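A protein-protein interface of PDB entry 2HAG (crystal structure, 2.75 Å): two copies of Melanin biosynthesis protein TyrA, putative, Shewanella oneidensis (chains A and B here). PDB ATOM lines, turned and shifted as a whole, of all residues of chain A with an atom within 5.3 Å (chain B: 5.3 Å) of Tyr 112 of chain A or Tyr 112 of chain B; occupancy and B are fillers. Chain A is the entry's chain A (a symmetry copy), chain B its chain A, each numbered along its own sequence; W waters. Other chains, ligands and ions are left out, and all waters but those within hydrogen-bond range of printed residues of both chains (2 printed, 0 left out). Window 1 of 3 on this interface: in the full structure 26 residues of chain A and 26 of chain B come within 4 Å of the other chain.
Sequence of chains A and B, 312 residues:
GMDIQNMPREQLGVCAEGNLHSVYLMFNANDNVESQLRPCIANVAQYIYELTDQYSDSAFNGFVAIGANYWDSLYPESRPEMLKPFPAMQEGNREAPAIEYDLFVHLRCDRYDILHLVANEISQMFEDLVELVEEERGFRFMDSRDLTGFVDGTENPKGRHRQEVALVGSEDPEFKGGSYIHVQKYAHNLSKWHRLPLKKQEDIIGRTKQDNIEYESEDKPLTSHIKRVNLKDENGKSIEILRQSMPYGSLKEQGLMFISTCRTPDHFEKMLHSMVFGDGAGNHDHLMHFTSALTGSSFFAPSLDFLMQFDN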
ATOM      1  N   HIS A  21      34.232  16.131 -10.924  1.00  0.00           N
ATOM      2  CA  HIS A  21      33.953  14.920 -10.181  1.00  0.00           C
ATOM      3  C   HIS A  21      35.226  14.260  -9.727  1.00  0.00           C
ATOM      4  O   HIS A  21      36.239  14.369 -10.390  1.00  0.00           O
ATOM      5  CB  HIS A  21      33.151  13.950 -11.043  1.00  0.00           C
ATOM      6  CG  HIS A  21      31.773  14.436 -11.382  1.00  0.00           C
ATOM      7  ND1 HIS A  21      31.407  14.809 -12.659  1.00  0.00           N
ATOM      8  CD2 HIS A  21      30.671  14.597 -10.614  1.00  0.00           C
ATOM      9  CE1 HIS A  21      30.139  15.177 -12.664  1.00  0.00           C
ATOM     10  NE2 HIS A  21      29.670  15.058 -11.437  1.00  0.00           N
ATOM     11  N   ASP A 110      36.032  15.310 -15.474  1.00  0.00           N
ATOM     12  CA  ASP A 110      34.873  16.166 -15.614  1.00  0.00           C
ATOM     13  C   ASP A 110      33.651  15.343 -15.968  1.00  0.00           C
ATOM     14  O   ASP A 110      32.541  15.855 -16.034  1.00  0.00           O
ATOM     15  CB  ASP A 110      35.138  17.259 -16.633  1.00  0.00           C
ATOM     16  CG  ASP A 110      36.047  18.341 -16.078  1.00  0.00           C
ATOM     17  OD1 ASP A 110      36.256  18.340 -14.835  1.00  0.00           O
ATOM     18  OD2 ASP A 110      36.541  19.188 -16.873  1.00  0.00           O
ATOM     19  N   ARG A 111      33.867  14.052 -16.170  1.00  0.00           N
ATOM     20  CA  ARG A 111      32.779  13.108 -16.324  1.00  0.00           C
ATOM     21  C   ARG A 111      32.813  12.045 -15.224  1.00  0.00           C
ATOM     22  O   ARG A 111      33.888  11.523 -14.878  1.00  0.00           O
ATOM     23  CB  ARG A 111      32.867  12.431 -17.676  1.00  0.00           C
ATOM     24  CG  ARG A 111      32.523  13.340 -18.823  1.00  0.00           C
ATOM     25  CD  ARG A 111      32.672  12.617 -20.158  1.00  0.00           C
ATOM     26  NE  ARG A 111      32.001  11.317 -20.167  1.00  0.00           N
ATOM     27  CZ  ARG A 111      31.782  10.604 -21.263  1.00  0.00           C
ATOM     28  NH1 ARG A 111      32.170  11.048 -22.436  1.00  0.00           N
ATOM     29  NH2 ARG A 111      31.165   9.444 -21.192  1.00  0.00           N
ATOM     30  N   TYR A 112      31.628  11.733 -14.697  1.00  0.00           N
ATOM     31  CA  TYR A 112      31.447  10.778 -13.600  1.00  0.00           C
ATOM     32  C   TYR A 112      31.513   9.349 -14.093  1.00  0.00           C
ATOM     33  O   TYR A 112      32.145   8.495 -13.484  1.00  0.00           O
ATOM     34  CB  TYR A 112      30.078  11.019 -12.996  1.00  0.00           C
ATOM     35  CG  TYR A 112      29.739  10.325 -11.702  1.00  0.00           C
ATOM     36  CD1 TYR A 112      29.467   8.961 -11.655  1.00  0.00           C
ATOM     37  CD2 TYR A 112      29.583  11.071 -10.529  1.00  0.00           C
ATOM     38  CE1 TYR A 112      29.102   8.355 -10.456  1.00  0.00           C
ATOM     39  CE2 TYR A 112      29.212  10.481  -9.332  1.00  0.00           C
ATOM     40  CZ  TYR A 112      28.977   9.132  -9.298  1.00  0.00           C
ATOM     41  OH  TYR A 112      28.607   8.594  -8.092  1.00  0.00           O
ATOM     42  N   ASP A 113      30.839   9.083 -15.200  1.00  0.00           N
ATOM     43  CA  ASP A 113      30.803   7.739 -15.749  1.00  0.00           C
ATOM     44  C   ASP A 113      32.221   7.228 -16.027  1.00  0.00           C
ATOM     45  O   ASP A 113      32.544   6.069 -15.764  1.00  0.00           O
ATOM     46  CB  ASP A 113      29.906   7.673 -16.991  1.00  0.00           C
ATOM     47  CG  ASP A 113      30.285   8.680 -18.073  1.00  0.00           C
ATOM     48  OD1 ASP A 113      31.256   9.445 -17.908  1.00  0.00           O
ATOM     49  OD2 ASP A 113      29.601   8.688 -19.120  1.00  0.00           O
ATOM     50  N   ILE A 114      33.084   8.101 -16.515  1.00  0.00           N
ATOM     51  CA  ILE A 114      34.442   7.683 -16.798  1.00  0.00           C
ATOM     52  C   ILE A 114      35.182   7.306 -15.524  1.00  0.00           C
ATOM     53  O   ILE A 114      35.865   6.284 -15.486  1.00  0.00           O
ATOM     54  CB  ILE A 114      35.185   8.754 -17.581  1.00  0.00           C
ATOM     55  CG1 ILE A 114      34.817   8.600 -19.050  1.00  0.00           C
ATOM     56  CG2 ILE A 114      36.676   8.616 -17.405  1.00  0.00           C
ATOM     57  CD1 ILE A 114      35.044   9.834 -19.848  1.00  0.00           C
ATOM     58  N   LEU A 115      35.026   8.110 -14.481  1.00  0.00           N
ATOM     59  CA  LEU A 115      35.609   7.786 -13.187  1.00  0.00           C
ATOM     60  C   LEU A 115      35.118   6.435 -12.669  1.00  0.00           C
ATOM     61  O   LEU A 115      35.859   5.707 -12.008  1.00  0.00           O
ATOM     62  CB  LEU A 115      35.275   8.880 -12.167  1.00  0.00           C
ATOM     63  CG  LEU A 115      36.097  10.174 -12.241  1.00  0.00           C
ATOM     64  CD1 LEU A 115      35.559  11.237 -11.277  1.00  0.00           C
ATOM     65  CD2 LEU A 115      37.568   9.913 -11.955  1.00  0.00           C
ATOM     66  N   HIS A 116      33.861   6.105 -12.957  1.00  0.00           N
ATOM     67  CA  HIS A 116      33.278   4.872 -12.448  1.00  0.00           C
ATOM     68  C   HIS A 116      33.965   3.704 -13.132  1.00  0.00           C
ATOM     69  O   HIS A 116      34.370   2.717 -12.500  1.00  0.00           O
ATOM     70  CB  HIS A 116      31.775   4.838 -12.728  1.00  0.00           C
ATOM     71  CG  HIS A 116      31.053   3.726 -12.033  1.00  0.00           C
ATOM     72  ND1 HIS A 116      30.476   3.873 -10.791  1.00  0.00           N
ATOM     73  CD2 HIS A 116      30.815   2.448 -12.406  1.00  0.00           C
ATOM     74  CE1 HIS A 116      29.918   2.733 -10.425  1.00  0.00           C
ATOM     75  NE2 HIS A 116      30.105   1.852 -11.391  1.00  0.00           N
ATOM     76  N   LEU A 117      34.087   3.838 -14.443  1.00  0.00           N
ATOM     77  CA  LEU A 117      34.780   2.858 -15.244  1.00  0.00           C
ATOM     78  C   LEU A 117      36.185   2.628 -14.719  1.00  0.00           C
ATOM     79  O   LEU A 117      36.591   1.488 -14.493  1.00  0.00           O
ATOM     80  CB  LEU A 117      34.872   3.354 -16.680  1.00  0.00           C
ATOM     81  CG  LEU A 117      35.680   2.470 -17.623  1.00  0.00           C
ATOM     82  CD1 LEU A 117      34.984   1.126 -17.777  1.00  0.00           C
ATOM     83  CD2 LEU A 117      35.851   3.154 -18.966  1.00  0.00           C
ATOM     84  N   ARG A 137      32.949   9.787  -3.133  1.00  0.00           N
ATOM     85  CA  ARG A 137      32.935  10.451  -4.420  1.00  0.00           C
ATOM     86  C   ARG A 137      32.655  11.905  -4.175  1.00  0.00           C
ATOM     87  O   ARG A 137      31.680  12.262  -3.503  1.00  0.00           O
ATOM     88  CB  ARG A 137      31.875   9.845  -5.342  1.00  0.00           C
ATOM     89  CG  ARG A 137      32.062   8.341  -5.505  1.00  0.00           C
ATOM     90  CD  ARG A 137      31.398   7.783  -6.758  1.00  0.00           C
ATOM     91  NE  ARG A 137      31.876   6.428  -7.048  1.00  0.00           N
ATOM     92  CZ  ARG A 137      31.599   5.736  -8.155  1.00  0.00           C
ATOM     93  NH1 ARG A 137      30.836   6.269  -9.108  1.00  0.00           N
ATOM     94  NH2 ARG A 137      32.100   4.509  -8.307  1.00  0.00           N
ATOM     95  N   PHE A 139      32.460  16.079  -5.659  1.00  0.00           N
ATOM     96  CA  PHE A 139      31.884  16.824  -6.757  1.00  0.00           C
ATOM     97  C   PHE A 139      32.124  18.306  -6.587  1.00  0.00           C
ATOM     98  O   PHE A 139      32.253  18.803  -5.465  1.00  0.00           O
ATOM     99  CB  PHE A 139      30.382  16.589  -6.802  1.00  0.00           C
ATOM    100  CG  PHE A 139      29.675  16.917  -5.515  1.00  0.00           C
ATOM    101  CD1 PHE A 139      29.575  15.970  -4.500  1.00  0.00           C
ATOM    102  CD2 PHE A 139      29.106  18.158  -5.322  1.00  0.00           C
ATOM    103  CE1 PHE A 139      28.928  16.257  -3.320  1.00  0.00           C
ATOM    104  CE2 PHE A 139      28.449  18.456  -4.141  1.00  0.00           C
ATOM    105  CZ  PHE A 139      28.363  17.507  -3.139  1.00  0.00           C
ATOM    106  N   GLY A 249      29.914  13.367  -0.421  1.00  0.00           N
ATOM    107  CA  GLY A 249      28.940  12.766   0.466  1.00  0.00           C
ATOM    108  C   GLY A 249      27.506  12.895   0.011  1.00  0.00           C
ATOM    109  O   GLY A 249      27.225  13.256  -1.137  1.00  0.00           O
ATOM    110  N   HIS B  21      22.276  12.676 -14.156  1.00  0.00           N
ATOM    111  CA  HIS B  21      22.421  12.344 -12.754  1.00  0.00           C
ATOM    112  C   HIS B  21      21.078  12.200 -12.092  1.00  0.00           C
ATOM    113  O   HIS B  21      20.131  12.852 -12.486  1.00  0.00           O
ATOM    114  CB  HIS B  21      23.232  13.421 -12.042  1.00  0.00           C
ATOM    115  CG  HIS B  21      24.659  13.506 -12.495  1.00  0.00           C
ATOM    116  ND1 HIS B  21      25.150  14.573 -13.219  1.00  0.00           N
ATOM    117  CD2 HIS B  21      25.702  12.663 -12.316  1.00  0.00           C
ATOM    118  CE1 HIS B  21      26.433  14.386 -13.465  1.00  0.00           C
ATOM    119  NE2 HIS B  21      26.793  13.235 -12.928  1.00  0.00           N
ATOM    120  N   ASP B 110      20.809  17.349 -14.955  1.00  0.00           N
ATOM    121  CA  ASP B 110      22.024  17.140 -15.714  1.00  0.00           C
ATOM    122  C   ASP B 110      23.220  17.665 -14.947  1.00  0.00           C
ATOM    123  O   ASP B 110      24.360  17.498 -15.361  1.00  0.00           O
ATOM    124  CB  ASP B 110      21.908  17.771 -17.090  1.00  0.00           C
ATOM    125  CG  ASP B 110      21.022  16.954 -18.014  1.00  0.00           C
ATOM    126  OD1 ASP B 110      20.712  15.791 -17.639  1.00  0.00           O
ATOM    127  OD2 ASP B 110      20.646  17.464 -19.105  1.00  0.00           O
ATOM    128  N   ARG B 111      22.946  18.281 -13.807  1.00  0.00           N
ATOM    129  CA  ARG B 111      23.985  18.663 -12.873  1.00  0.00           C
ATOM    130  C   ARG B 111      23.799  17.964 -11.525  1.00  0.00           C
ATOM    131  O   ARG B 111      22.670  17.867 -11.011  1.00  0.00           O
ATOM    132  CB  ARG B 111      23.969  20.163 -12.665  1.00  0.00           C
ATOM    133  CG  ARG B 111      24.458  20.938 -13.856  1.00  0.00           C
ATOM    134  CD  ARG B 111      24.376  22.441 -13.604  1.00  0.00           C
ATOM    135  NE  ARG B 111      24.968  22.824 -12.322  1.00  0.00           N
ATOM    136  CZ  ARG B 111      25.234  24.076 -11.974  1.00  0.00           C
ATOM    137  NH1 ARG B 111      24.970  25.066 -12.793  1.00  0.00           N
ATOM    138  NH2 ARG B 111      25.774  24.342 -10.804  1.00  0.00           N
ATOM    139  N   TYR B 112      24.916  17.496 -10.967  1.00  0.00           N
ATOM    140  CA  TYR B 112      24.950  16.751  -9.705  1.00  0.00           C
ATOM    141  C   TYR B 112      24.840  17.678  -8.513  1.00  0.00           C
ATOM    142  O   TYR B 112      24.111  17.412  -7.567  1.00  0.00           O
ATOM    143  CB  TYR B 112      26.276  16.023  -9.631  1.00  0.00           C
ATOM    144  CG  TYR B 112      26.467  15.001  -8.540  1.00  0.00           C
ATOM    145  CD1 TYR B 112      26.653  15.375  -7.213  1.00  0.00           C
ATOM    146  CD2 TYR B 112      26.570  13.643  -8.865  1.00  0.00           C
ATOM    147  CE1 TYR B 112      26.882  14.413  -6.234  1.00  0.00           C
ATOM    148  CE2 TYR B 112      26.806  12.678  -7.901  1.00  0.00           C
ATOM    149  CZ  TYR B 112      26.958  13.062  -6.595  1.00  0.00           C
ATOM    150  OH  TYR B 112      27.195  12.072  -5.677  1.00  0.00           O
ATOM    151  N   ASP B 113      25.585  18.770  -8.554  1.00  0.00           N
ATOM    152  CA  ASP B 113      25.587  19.716  -7.452  1.00  0.00           C
ATOM    153  C   ASP B 113      24.169  20.226  -7.173  1.00  0.00           C
ATOM    154  O   ASP B 113      23.758  20.366  -6.019  1.00  0.00           O
ATOM    155  CB  ASP B 113      26.578  20.859  -7.706  1.00  0.00           C
ATOM    156  CG  ASP B 113      26.348  21.583  -9.029  1.00  0.00           C
ATOM    157  OD1 ASP B 113      25.414  21.241  -9.781  1.00  0.00           O
ATOM    158  OD2 ASP B 113      27.115  22.531  -9.310  1.00  0.00           O
ATOM    159  N   ILE B 114      23.402  20.460  -8.221  1.00  0.00           N
ATOM    160  CA  ILE B 114      22.049  20.941  -8.027  1.00  0.00           C
ATOM    161  C   ILE B 114      21.186  19.900  -7.330  1.00  0.00           C
ATOM    162  O   ILE B 114      20.444  20.230  -6.408  1.00  0.00           O
ATOM    163  CB  ILE B 114      21.438  21.383  -9.346  1.00  0.00           C
ATOM    164  CG1 ILE B 114      21.914  22.800  -9.632  1.00  0.00           C
ATOM    165  CG2 ILE B 114      19.931  21.349  -9.283  1.00  0.00           C
ATOM    166  CD1 ILE B 114      21.827  23.175 -11.069  1.00  0.00           C
ATOM    167  N   LEU B 115      21.304  18.648  -7.751  1.00  0.00           N
ATOM    168  CA  LEU B 115      20.599  17.561  -7.086  1.00  0.00           C
ATOM    169  C   LEU B 115      20.965  17.473  -5.606  1.00  0.00           C
ATOM    170  O   LEU B 115      20.130  17.124  -4.770  1.00  0.00           O
ATOM    171  CB  LEU B 115      20.912  16.228  -7.773  1.00  0.00           C
ATOM    172  CG  LEU B 115      20.176  15.934  -9.088  1.00  0.00           C
ATOM    173  CD1 LEU B 115      20.695  14.651  -9.746  1.00  0.00           C
ATOM    174  CD2 LEU B 115      18.674  15.833  -8.872  1.00  0.00           C
ATOM    175  N   HIS B 116      22.219  17.777  -5.281  1.00  0.00           N
ATOM    176  CA  HIS B 116      22.686  17.655  -3.906  1.00  0.00           C
ATOM    177  C   HIS B 116      21.989  18.715  -3.073  1.00  0.00           C
ATOM    178  O   HIS B 116      21.476  18.456  -1.974  1.00  0.00           O
ATOM    179  CB  HIS B 116      24.202  17.841  -3.839  1.00  0.00           C
ATOM    180  CG  HIS B 116      24.798  17.497  -2.510  1.00  0.00           C
ATOM    181  ND1 HIS B 116      25.279  16.241  -2.212  1.00  0.00           N
ATOM    182  CD2 HIS B 116      24.990  18.244  -1.399  1.00  0.00           C
ATOM    183  CE1 HIS B 116      25.736  16.225  -0.973  1.00  0.00           C
ATOM    184  NE2 HIS B 116      25.577  17.431  -0.458  1.00  0.00           N
ATOM    185  N   LEU B 117      21.982  19.920  -3.621  1.00  0.00           N
ATOM    186  CA  LEU B 117      21.302  21.030  -3.003  1.00  0.00           C
ATOM    187  C   LEU B 117      19.847  20.690  -2.735  1.00  0.00           C
ATOM    188  O   LEU B 117      19.357  20.864  -1.620  1.00  0.00           O
ATOM    189  CB  LEU B 117      21.356  22.236  -3.930  1.00  0.00           C
ATOM    190  CG  LEU B 117      20.578  23.457  -3.457  1.00  0.00           C
ATOM    191  CD1 LEU B 117      21.203  23.991  -2.177  1.00  0.00           C
ATOM    192  CD2 LEU B 117      20.559  24.520  -4.539  1.00  0.00           C
ATOM    193  N   ARG B 137      22.540   7.256  -5.604  1.00  0.00           N
ATOM    194  CA  ARG B 137      22.698   8.261  -6.635  1.00  0.00           C
ATOM    195  C   ARG B 137      23.042   7.548  -7.911  1.00  0.00           C
ATOM    196  O   ARG B 137      23.978   6.741  -7.957  1.00  0.00           O
ATOM    197  CB  ARG B 137      23.792   9.264  -6.264  1.00  0.00           C
ATOM    198  CG  ARG B 137      23.531   9.909  -4.909  1.00  0.00           C
ATOM    199  CD  ARG B 137      24.262  11.233  -4.720  1.00  0.00           C
ATOM    200  NE  ARG B 137      23.729  11.967  -3.568  1.00  0.00           N
ATOM    201  CZ  ARG B 137      24.055  13.219  -3.239  1.00  0.00           C
ATOM    202  NH1 ARG B 137      24.924  13.906  -3.979  1.00  0.00           N
ATOM    203  NH2 ARG B 137      23.497  13.785  -2.166  1.00  0.00           N
ATOM    204  N   PHE B 139      23.604   7.609 -12.308  1.00  0.00           N
ATOM    205  CA  PHE B 139      24.311   8.376 -13.310  1.00  0.00           C
ATOM    206  C   PHE B 139      24.145   7.756 -14.679  1.00  0.00           C
ATOM    207  O   PHE B 139      23.954   6.544 -14.807  1.00  0.00           O
ATOM    208  CB  PHE B 139      25.795   8.405 -12.979  1.00  0.00           C
ATOM    209  CG  PHE B 139      26.412   7.041 -12.828  1.00  0.00           C
ATOM    210  CD1 PHE B 139      26.373   6.378 -11.605  1.00  0.00           C
ATOM    211  CD2 PHE B 139      27.035   6.429 -13.894  1.00  0.00           C
ATOM    212  CE1 PHE B 139      26.936   5.131 -11.453  1.00  0.00           C
ATOM    213  CE2 PHE B 139      27.610   5.178 -13.752  1.00  0.00           C
ATOM    214  CZ  PHE B 139      27.557   4.528 -12.532  1.00  0.00           C
ATOM    215  N   GLY B 249      25.548   3.370  -7.890  1.00  0.00           N
ATOM    216  CA  GLY B 249      26.409   2.665  -6.963  1.00  0.00           C
ATOM    217  C   GLY B 249      27.881   2.969  -7.110  1.00  0.00           C
ATOM    218  O   GLY B 249      28.275   3.924  -7.790  1.00  0.00           O
HETATM  219  O   HOH W   1      26.821   6.340  -8.268  1.00  0.00           O
HETATM  220  O   HOH W   2      28.853  12.852  -3.454  1.00  0.00           O
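The side-chain hydroxyl (OH) of Tyr 112 of chain B lies close to the guanidinium group (NH1) of Arg 137 of chain B (3.4 Å).
OH of Tyr 112 of chain A sits close to NH1 of Arg 137 of chain A (3.4 Å).
ND1 of His 116 of chain B sits at hydrogen-bond distance from NH1 of Arg 137 of chain B.
The guanidinium group (NH1) of Arg 137 of chain A sits at hydrogen-bond distance from a ring nitrogen (ND1) of His 116 of chain A.
Water W2 lies within hydrogen-bond range of O of Gly 249 of chain A, OH of Tyr 112 of chain B and O of Arg 137 of chain A.
Water W1 lies within hydrogen-bond range of the backbone carbonyl oxygen (O) of Gly 249 of chain B (2.9 Å), the side-chain hydroxyl (OH) of Tyr 112 of chain A (2.9 Å) and the backbone carbonyl oxygen (O) of Arg 137 of chain B (2.9 Å).
NE2 of His 21 of chain A touches NE2 of His 21 of chain B (3.7 Å).
His 21 of chain B touches Tyr 112 of chain A.
Tyr 112 of chain B touches Tyr 112 of chain A (CE2 to CE2, 3.6 Å).
Phe 139 of chain B touches Tyr 112 of chain A (CD1 to CE1, 3.6 Å).
His 116 of chain A touches Phe 139 of chain B (ND1 to CZ, 3.5 Å).
O of Gly 249 of chain B touches CE1 of His 116 of chain A, at 3.3 Å.
Arg 137 of chain A touches Gly 249 of chain B.
CD1 of Phe 139 of chain A touches CE1 of Tyr 112 of chain B (3.6 Å).
CE1 of His 116 of chain B touches O of Gly 249 of chain A, 3.3 Å away.
Arg 137 of chain B touches Gly 249 of chain A.
Of the printed residues of chain B, His 21 of chain A touches His 21 and Tyr 112.
Printed residues of chain B within 4 Å of Tyr 112 of chain A: His 21, Tyr 112 and Phe 139.
Printed residues of chain B within 4 Å of Gly 249 of chain A: His 116 (3.3 Å) and Arg 137 (3.7 Å).
Of chain A, only His 21 (3.96 Å), Tyr 112 (3.6 Å) and Phe 139 (3.6 Å) come within 4 Å of Tyr 112 of chain B.
Printed residues of chain A within 4 Å of His 116 of chain B: Phe 139 and Gly 249.
Of the printed residues of chain A, Arg 137 of chain B touches Gly 249 (3.7 Å).
Printed residues of chain A within 4 Å of Gly 249 of chain B: His 116 (3.3 Å) and Arg 137 (3.7 Å).
The nearest residue of chain B that does not touch Tyr 112 of chain A is Gly 249 of chain B (4.7 Å).
The nearest printed residue of chain A that does not touch His 21 of chain B is Asp 113 of chain A (6.2 Å).
Of the 12 printed residues of chain A, 6 touch a printed residue of chain B.
Hydrophobic or aromatic side chains of chain A within 4 Å of the printed part of chain B: His 21, Tyr 112, His 116 and Phe 139.
Tyr 112 of chain A touches its own counterpart, Tyr 112 of chain B.
Tyr 112 of chain A touches Phe 139 of chain B, and with the chains exchanged Phe 139 of chain A touches Tyr 112 of chain B.
His 116 of chain A touches Phe 139 of chain B, and with the chains exchanged Phe 139 of chain A touches His 116 of chain B.
His 116 of chain A touches Gly 249 of chain B, and with the chains exchanged Gly 249 of chain A touches His 116 of chain B.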
